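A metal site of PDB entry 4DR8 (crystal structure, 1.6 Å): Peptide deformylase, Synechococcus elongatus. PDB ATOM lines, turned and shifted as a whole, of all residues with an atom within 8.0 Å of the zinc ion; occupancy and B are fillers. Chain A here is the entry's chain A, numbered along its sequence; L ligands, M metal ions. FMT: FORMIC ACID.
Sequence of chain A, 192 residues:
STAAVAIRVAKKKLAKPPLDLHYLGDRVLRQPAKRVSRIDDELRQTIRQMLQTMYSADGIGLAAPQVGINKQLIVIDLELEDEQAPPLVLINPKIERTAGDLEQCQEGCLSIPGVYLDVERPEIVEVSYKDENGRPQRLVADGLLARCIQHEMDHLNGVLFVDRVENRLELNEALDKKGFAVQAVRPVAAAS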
ATOM      1  N   LEU A  29      17.951 -11.337  18.019  1.00  0.00           N
ATOM      2  CA  LEU A  29      17.157 -10.260  17.513  1.00  0.00           C
ATOM      3  C   LEU A  29      16.416  -9.502  18.622  1.00  0.00           C
ATOM      4  O   LEU A  29      15.795  -8.470  18.373  1.00  0.00           O
ATOM      5  CB  LEU A  29      16.180 -10.773  16.478  1.00  0.00           C
ATOM      6  CG  LEU A  29      16.780 -11.470  15.263  1.00  0.00           C
ATOM      7  CD1 LEU A  29      15.685 -12.028  14.374  1.00  0.00           C
ATOM      8  CD2 LEU A  29      17.669 -10.496  14.474  1.00  0.00           C
ATOM      9  N   GLY A  61      18.124  -2.033   4.213  1.00  0.00           N
ATOM     10  CA  GLY A  61      18.708  -1.694   5.508  1.00  0.00           C
ATOM     11  C   GLY A  61      19.115  -2.963   6.229  1.00  0.00           C
ATOM     12  O   GLY A  61      18.620  -4.065   5.972  1.00  0.00           O
ATOM     13  N   LEU A  62      20.059  -2.807   7.150  1.00  0.00           N
ATOM     14  CA  LEU A  62      20.560  -3.961   7.920  1.00  0.00           C
ATOM     15  C   LEU A  62      21.178  -3.378   9.196  1.00  0.00           C
ATOM     16  O   LEU A  62      22.010  -2.468   9.160  1.00  0.00           O
ATOM     17  CB  LEU A  62      21.566  -4.818   7.131  1.00  0.00           C
ATOM     18  CG  LEU A  62      22.117  -6.027   7.826  1.00  0.00           C
ATOM     19  CD1 LEU A  62      21.048  -7.124   7.920  1.00  0.00           C
ATOM     20  CD2 LEU A  62      23.312  -6.597   7.023  1.00  0.00           C
ATOM     21  N   ALA A  63      20.730  -3.916  10.319  1.00  0.00           N
ATOM     22  CA  ALA A  63      21.190  -3.610  11.648  1.00  0.00           C
ATOM     23  C   ALA A  63      22.108  -4.738  12.109  1.00  0.00           C
ATOM     24  O   ALA A  63      21.826  -5.937  11.848  1.00  0.00           O
ATOM     25  CB  ALA A  63      20.001  -3.518  12.606  1.00  0.00           C
ATOM     26  N   GLN A  66      21.062  -8.308  13.373  1.00  0.00           N
ATOM     27  CA  GLN A  66      20.538  -9.228  12.391  1.00  0.00           C
ATOM     28  C   GLN A  66      21.581 -10.187  11.858  1.00  0.00           C
ATOM     29  O   GLN A  66      21.213 -11.237  11.348  1.00  0.00           O
ATOM     30  CB  GLN A  66      19.921  -8.524  11.213  1.00  0.00           C
ATOM     31  CG  GLN A  66      18.757  -7.653  11.561  1.00  0.00           C
ATOM     32  CD  GLN A  66      18.173  -6.979  10.358  1.00  0.00           C
ATOM     33  OE1 GLN A  66      18.413  -5.780  10.120  1.00  0.00           O
ATOM     34  NE2 GLN A  66      17.439  -7.743   9.530  1.00  0.00           N
ATOM     35  N   GLU A 107       5.804  -3.354   5.100  1.00  0.00           N
ATOM     36  CA  GLU A 107       7.226  -3.563   5.375  1.00  0.00           C
ATOM     37  C   GLU A 107       7.608  -5.036   5.243  1.00  0.00           C
ATOM     38  O   GLU A 107       6.773  -5.920   5.458  1.00  0.00           O
ATOM     39  CB  GLU A 107       7.588  -3.093   6.787  1.00  0.00           C
ATOM     40  CG  GLU A 107       7.476  -1.593   6.947  1.00  0.00           C
ATOM     41  CD  GLU A 107       7.962  -1.089   8.279  1.00  0.00           C
ATOM     42  OE1 GLU A 107       8.813  -1.728   8.932  1.00  0.00           O
ATOM     43  OE2 GLU A 107       7.458  -0.016   8.689  1.00  0.00           O
ATOM     44  N   GLY A 108       8.884  -5.277   4.941  1.00  0.00           N
ATOM     45  CA  GLY A 108       9.480  -6.579   5.060  1.00  0.00           C
ATOM     46  C   GLY A 108      10.736  -6.440   5.903  1.00  0.00           C
ATOM     47  O   GLY A 108      11.063  -5.360   6.362  1.00  0.00           O
ATOM     48  N   CYS A 109      11.446  -7.535   6.058  1.00  0.00           N
ATOM     49  CA  CYS A 109      12.675  -7.530   6.832  1.00  0.00           C
ATOM     50  C   CYS A 109      13.551  -8.709   6.439  1.00  0.00           C
ATOM     51  O   CYS A 109      13.052  -9.816   6.299  1.00  0.00           O
ATOM     52  CB  CYS A 109      12.347  -7.659   8.344  1.00  0.00           C
ATOM     53  SG  CYS A 109      13.736  -7.676   9.515  1.00  0.00           S
ATOM     54  N   LEU A 110      14.872  -8.498   6.355  1.00  0.00           N
ATOM     55  CA  LEU A 110      15.783  -9.594   6.034  1.00  0.00           C
ATOM     56  C   LEU A 110      15.811 -10.686   7.094  1.00  0.00           C
ATOM     57  O   LEU A 110      16.172 -11.832   6.790  1.00  0.00           O
ATOM     58  CB  LEU A 110      17.188  -9.075   5.828  1.00  0.00           C
ATOM     59  CG  LEU A 110      17.417  -8.207   4.589  1.00  0.00           C
ATOM     60  CD1 LEU A 110      18.927  -7.973   4.473  1.00  0.00           C
ATOM     61  CD2 LEU A 110      16.870  -8.819   3.337  1.00  0.00           C
ATOM     62  N   SER A 111      15.398 -10.368   8.313  1.00  0.00           N
ATOM     63  CA  SER A 111      15.323 -11.338   9.397  1.00  0.00           C
ATOM     64  C   SER A 111      13.961 -12.018   9.491  1.00  0.00           C
ATOM     65  O   SER A 111      13.783 -12.940  10.315  1.00  0.00           O
ATOM     66  CB  SER A 111      15.671 -10.690  10.723  1.00  0.00           C
ATOM     67  OG  SER A 111      17.002 -10.364  10.776  1.00  0.00           O
ATOM     68  N   ILE A 112      13.016 -11.616   8.649  1.00  0.00           N
ATOM     69  CA  ILE A 112      11.725 -12.256   8.575  1.00  0.00           C
ATOM     70  C   ILE A 112      11.371 -12.479   7.123  1.00  0.00           C
ATOM     71  O   ILE A 112      10.384 -11.955   6.625  1.00  0.00           O
ATOM     72  CB  ILE A 112      10.615 -11.485   9.317  1.00  0.00           C
ATOM     73  CG1 ILE A 112      11.161 -10.896  10.618  1.00  0.00           C
ATOM     74  CG2 ILE A 112       9.456 -12.430   9.605  1.00  0.00           C
ATOM     75  CD1 ILE A 112      10.185 -10.071  11.419  1.00  0.00           C
ATOM     76  N   ARG A 121       3.708   4.076  11.283  1.00  0.00           N
ATOM     77  CA  ARG A 121       4.828   4.818  11.928  1.00  0.00           C
ATOM     78  C   ARG A 121       4.667   6.296  11.605  1.00  0.00           C
ATOM     79  O   ARG A 121       4.051   6.667  10.599  1.00  0.00           O
ATOM     80  CB  ARG A 121       6.190   4.403  11.391  1.00  0.00           C
ATOM     81  CG  ARG A 121       6.501   2.921  11.467  1.00  0.00           C
ATOM     82  CD  ARG A 121       7.959   2.669  11.118  1.00  0.00           C
ATOM     83  NE  ARG A 121       8.301   1.258  10.952  1.00  0.00           N
ATOM     84  CZ  ARG A 121       8.865   0.512  11.881  1.00  0.00           C
ATOM     85  NH1 ARG A 121       9.168   1.000  13.071  1.00  0.00           N
ATOM     86  NH2 ARG A 121       9.139  -0.750  11.604  1.00  0.00           N
ATOM     87  N   CYS A 148      12.582   3.354   6.995  1.00  0.00           N
ATOM     88  CA  CYS A 148      13.714   2.394   7.131  1.00  0.00           C
ATOM     89  C   CYS A 148      14.571   2.732   8.376  1.00  0.00           C
ATOM     90  O   CYS A 148      14.904   1.848   9.148  1.00  0.00           O
ATOM     91  CB  CYS A 148      14.547   2.476   5.865  1.00  0.00           C
ATOM     92  SG  CYS A 148      15.932   1.324   5.773  1.00  0.00           S
ATOM     93  N   HIS A 151      12.544   1.456  11.411  1.00  0.00           N
ATOM     94  CA  HIS A 151      12.631  -0.015  11.396  1.00  0.00           C
ATOM     95  C   HIS A 151      13.990  -0.476  11.910  1.00  0.00           C
ATOM     96  O   HIS A 151      14.100  -1.384  12.720  1.00  0.00           O
ATOM     97  CB  HIS A 151      12.345  -0.490   9.968  1.00  0.00           C
ATOM     98  CG  HIS A 151      12.490  -1.978   9.767  1.00  0.00           C
ATOM     99  ND1 HIS A 151      11.467  -2.767   9.284  1.00  0.00           N
ATOM    100  CD2 HIS A 151      13.581  -2.773   9.934  1.00  0.00           C
ATOM    101  CE1 HIS A 151      11.935  -4.031   9.180  1.00  0.00           C
ATOM    102  NE2 HIS A 151      13.213  -4.030   9.589  1.00  0.00           N
ATOM    103  N   GLU A 152      15.051   0.114  11.395  1.00  0.00           N
ATOM    104  CA  GLU A 152      16.389  -0.297  11.798  1.00  0.00           C
ATOM    105  C   GLU A 152      16.742   0.106  13.214  1.00  0.00           C
ATOM    106  O   GLU A 152      17.396  -0.645  13.938  1.00  0.00           O
ATOM    107  CB  GLU A 152      17.427   0.227  10.795  1.00  0.00           C
ATOM    108  CG  GLU A 152      17.322  -0.335   9.377  1.00  0.00           C
ATOM    109  CD  GLU A 152      17.219  -1.825   9.247  1.00  0.00           C
ATOM    110  OE1 GLU A 152      17.842  -2.516  10.080  1.00  0.00           O
ATOM    111  OE2 GLU A 152      16.566  -2.259   8.239  1.00  0.00           O
ATOM    112  N   ASP A 154      14.538   0.230  15.549  1.00  0.00           N
ATOM    113  CA  ASP A 154      13.838  -0.816  16.307  1.00  0.00           C
ATOM    114  C   ASP A 154      14.741  -2.057  16.521  1.00  0.00           C
ATOM    115  O   ASP A 154      14.762  -2.613  17.610  1.00  0.00           O
ATOM    116  CB  ASP A 154      12.534  -1.206  15.582  1.00  0.00           C
ATOM    117  CG  ASP A 154      11.308  -0.359  15.975  1.00  0.00           C
ATOM    118  OD1 ASP A 154      11.311   0.437  16.936  1.00  0.00           O
ATOM    119  OD2 ASP A 154      10.287  -0.591  15.297  1.00  0.00           O
ATOM    120  N   HIS A 155      15.502  -2.463  15.498  1.00  0.00           N
ATOM    121  CA  HIS A 155      16.377  -3.627  15.647  1.00  0.00           C
ATOM    122  C   HIS A 155      17.371  -3.419  16.773  1.00  0.00           C
ATOM    123  O   HIS A 155      17.750  -4.347  17.471  1.00  0.00           O
ATOM    124  CB  HIS A 155      17.125  -3.976  14.362  1.00  0.00           C
ATOM    125  CG  HIS A 155      16.317  -4.705  13.317  1.00  0.00           C
ATOM    126  ND1 HIS A 155      15.837  -5.965  13.540  1.00  0.00           N
ATOM    127  CD2 HIS A 155      16.031  -4.412  12.017  1.00  0.00           C
ATOM    128  CE1 HIS A 155      15.214  -6.397  12.438  1.00  0.00           C
ATOM    129  NE2 HIS A 155      15.300  -5.450  11.510  1.00  0.00           N
ATOM    130  N   VAL A 159      13.433  -4.882  18.820  1.00  0.00           N
ATOM    131  CA  VAL A 159      12.032  -4.733  18.350  1.00  0.00           C
ATOM    132  C   VAL A 159      11.994  -5.080  16.890  1.00  0.00           C
ATOM    133  O   VAL A 159      12.860  -4.655  16.136  1.00  0.00           O
ATOM    134  CB  VAL A 159      11.505  -3.303  18.585  1.00  0.00           C
ATOM    135  CG1 VAL A 159      10.105  -3.097  18.005  1.00  0.00           C
ATOM    136  CG2 VAL A 159      11.534  -2.970  20.063  1.00  0.00           C
ATOM    137  N   LEU A 160      11.008  -5.913  16.530  1.00  0.00           N
ATOM    138  CA  LEU A 160      10.824  -6.419  15.156  1.00  0.00           C
ATOM    139  C   LEU A 160       9.500  -5.893  14.638  1.00  0.00           C
ATOM    140  O   LEU A 160       8.567  -5.623  15.417  1.00  0.00           O
ATOM    141  CB  LEU A 160      10.881  -7.953  15.154  1.00  0.00           C
ATOM    142  CG  LEU A 160      12.212  -8.560  15.612  1.00  0.00           C
ATOM    143  CD1 LEU A 160      12.135 -10.080  15.700  1.00  0.00           C
ATOM    144  CD2 LEU A 160      13.367  -8.094  14.715  1.00  0.00           C
ATOM    145  N   PHE A 161       9.389  -5.752  13.337  1.00  0.00           N
ATOM    146  CA  PHE A 161       8.241  -5.027  12.768  1.00  0.00           C
ATOM    147  C   PHE A 161       6.922  -5.739  13.003  1.00  0.00           C
ATOM    148  O   PHE A 161       5.891  -5.080  13.131  1.00  0.00           O
ATOM    149  CB  PHE A 161       8.406  -4.680  11.297  1.00  0.00           C
ATOM    150  CG  PHE A 161       8.123  -5.793  10.322  1.00  0.00           C
ATOM    151  CD1 PHE A 161       9.111  -6.679   9.908  1.00  0.00           C
ATOM    152  CD2 PHE A 161       6.876  -5.883   9.739  1.00  0.00           C
ATOM    153  CE1 PHE A 161       8.810  -7.682   8.949  1.00  0.00           C
ATOM    154  CE2 PHE A 161       6.606  -6.834   8.802  1.00  0.00           C
ATOM    155  CZ  PHE A 161       7.565  -7.720   8.403  1.00  0.00           C
HETATM  156  C   FMT L   1      15.730  -5.516   7.560  1.00  0.00           C
HETATM  157  O1  FMT L   1      16.561  -5.957   6.767  1.00  0.00           O
HETATM  158  O2  FMT L   1      16.088  -4.854   8.573  1.00  0.00           O
HETATM  159 ZN    ZN M   1      14.507  -5.567   9.645  1.00  0.00          ZN
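OG of Ser 111 sits at hydrogen-bond distance from NE2 of Gln 66, 2.9 Å away.
The side-chain sulfur of Cys 109 lies close to the backbone NH of Ser 111.
The side-chain amide oxygen (OE1) of Gln 66 lies close to the side-chain carboxylate (OE1) of Glu 152 (3.3 Å).
A ring nitrogen (ND1) of His 151 is in hydrogen-bond range of the side-chain carboxylate (OE1) of Glu 107, 2.9 Å away.
OE1 of Gln 66 lies close to NE2 of His 155.
The side-chain sulfur (SG) of Cys 109 sits close to the side-chain amide nitrogen (NE2) of Gln 66, at 3.7 Å.
The side-chain amide oxygen (OE1) of Gln 66 is in hydrogen-bond range of the backbone NH (N) of Ala 63 (3.0 Å).
Gln 66 touches the zinc ion.
Of the 20 residues printed, 4 come within 4 Å of the zinc ion.
The nearest printed residue that does not touch the zinc ion is Glu 152 (4.1 Å).
The zinc ion is bound by a ring nitrogen (NE2) of His 151 (2.0 Å), a ring nitrogen (NE2) of His 155 (2.0 Å), an oxygen (O2) of the ligand (2.0 Å) and the side-chain sulfur (SG) of Cys 109 (2.2 Å).
The zinc ion has four donor atoms within binding distance.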
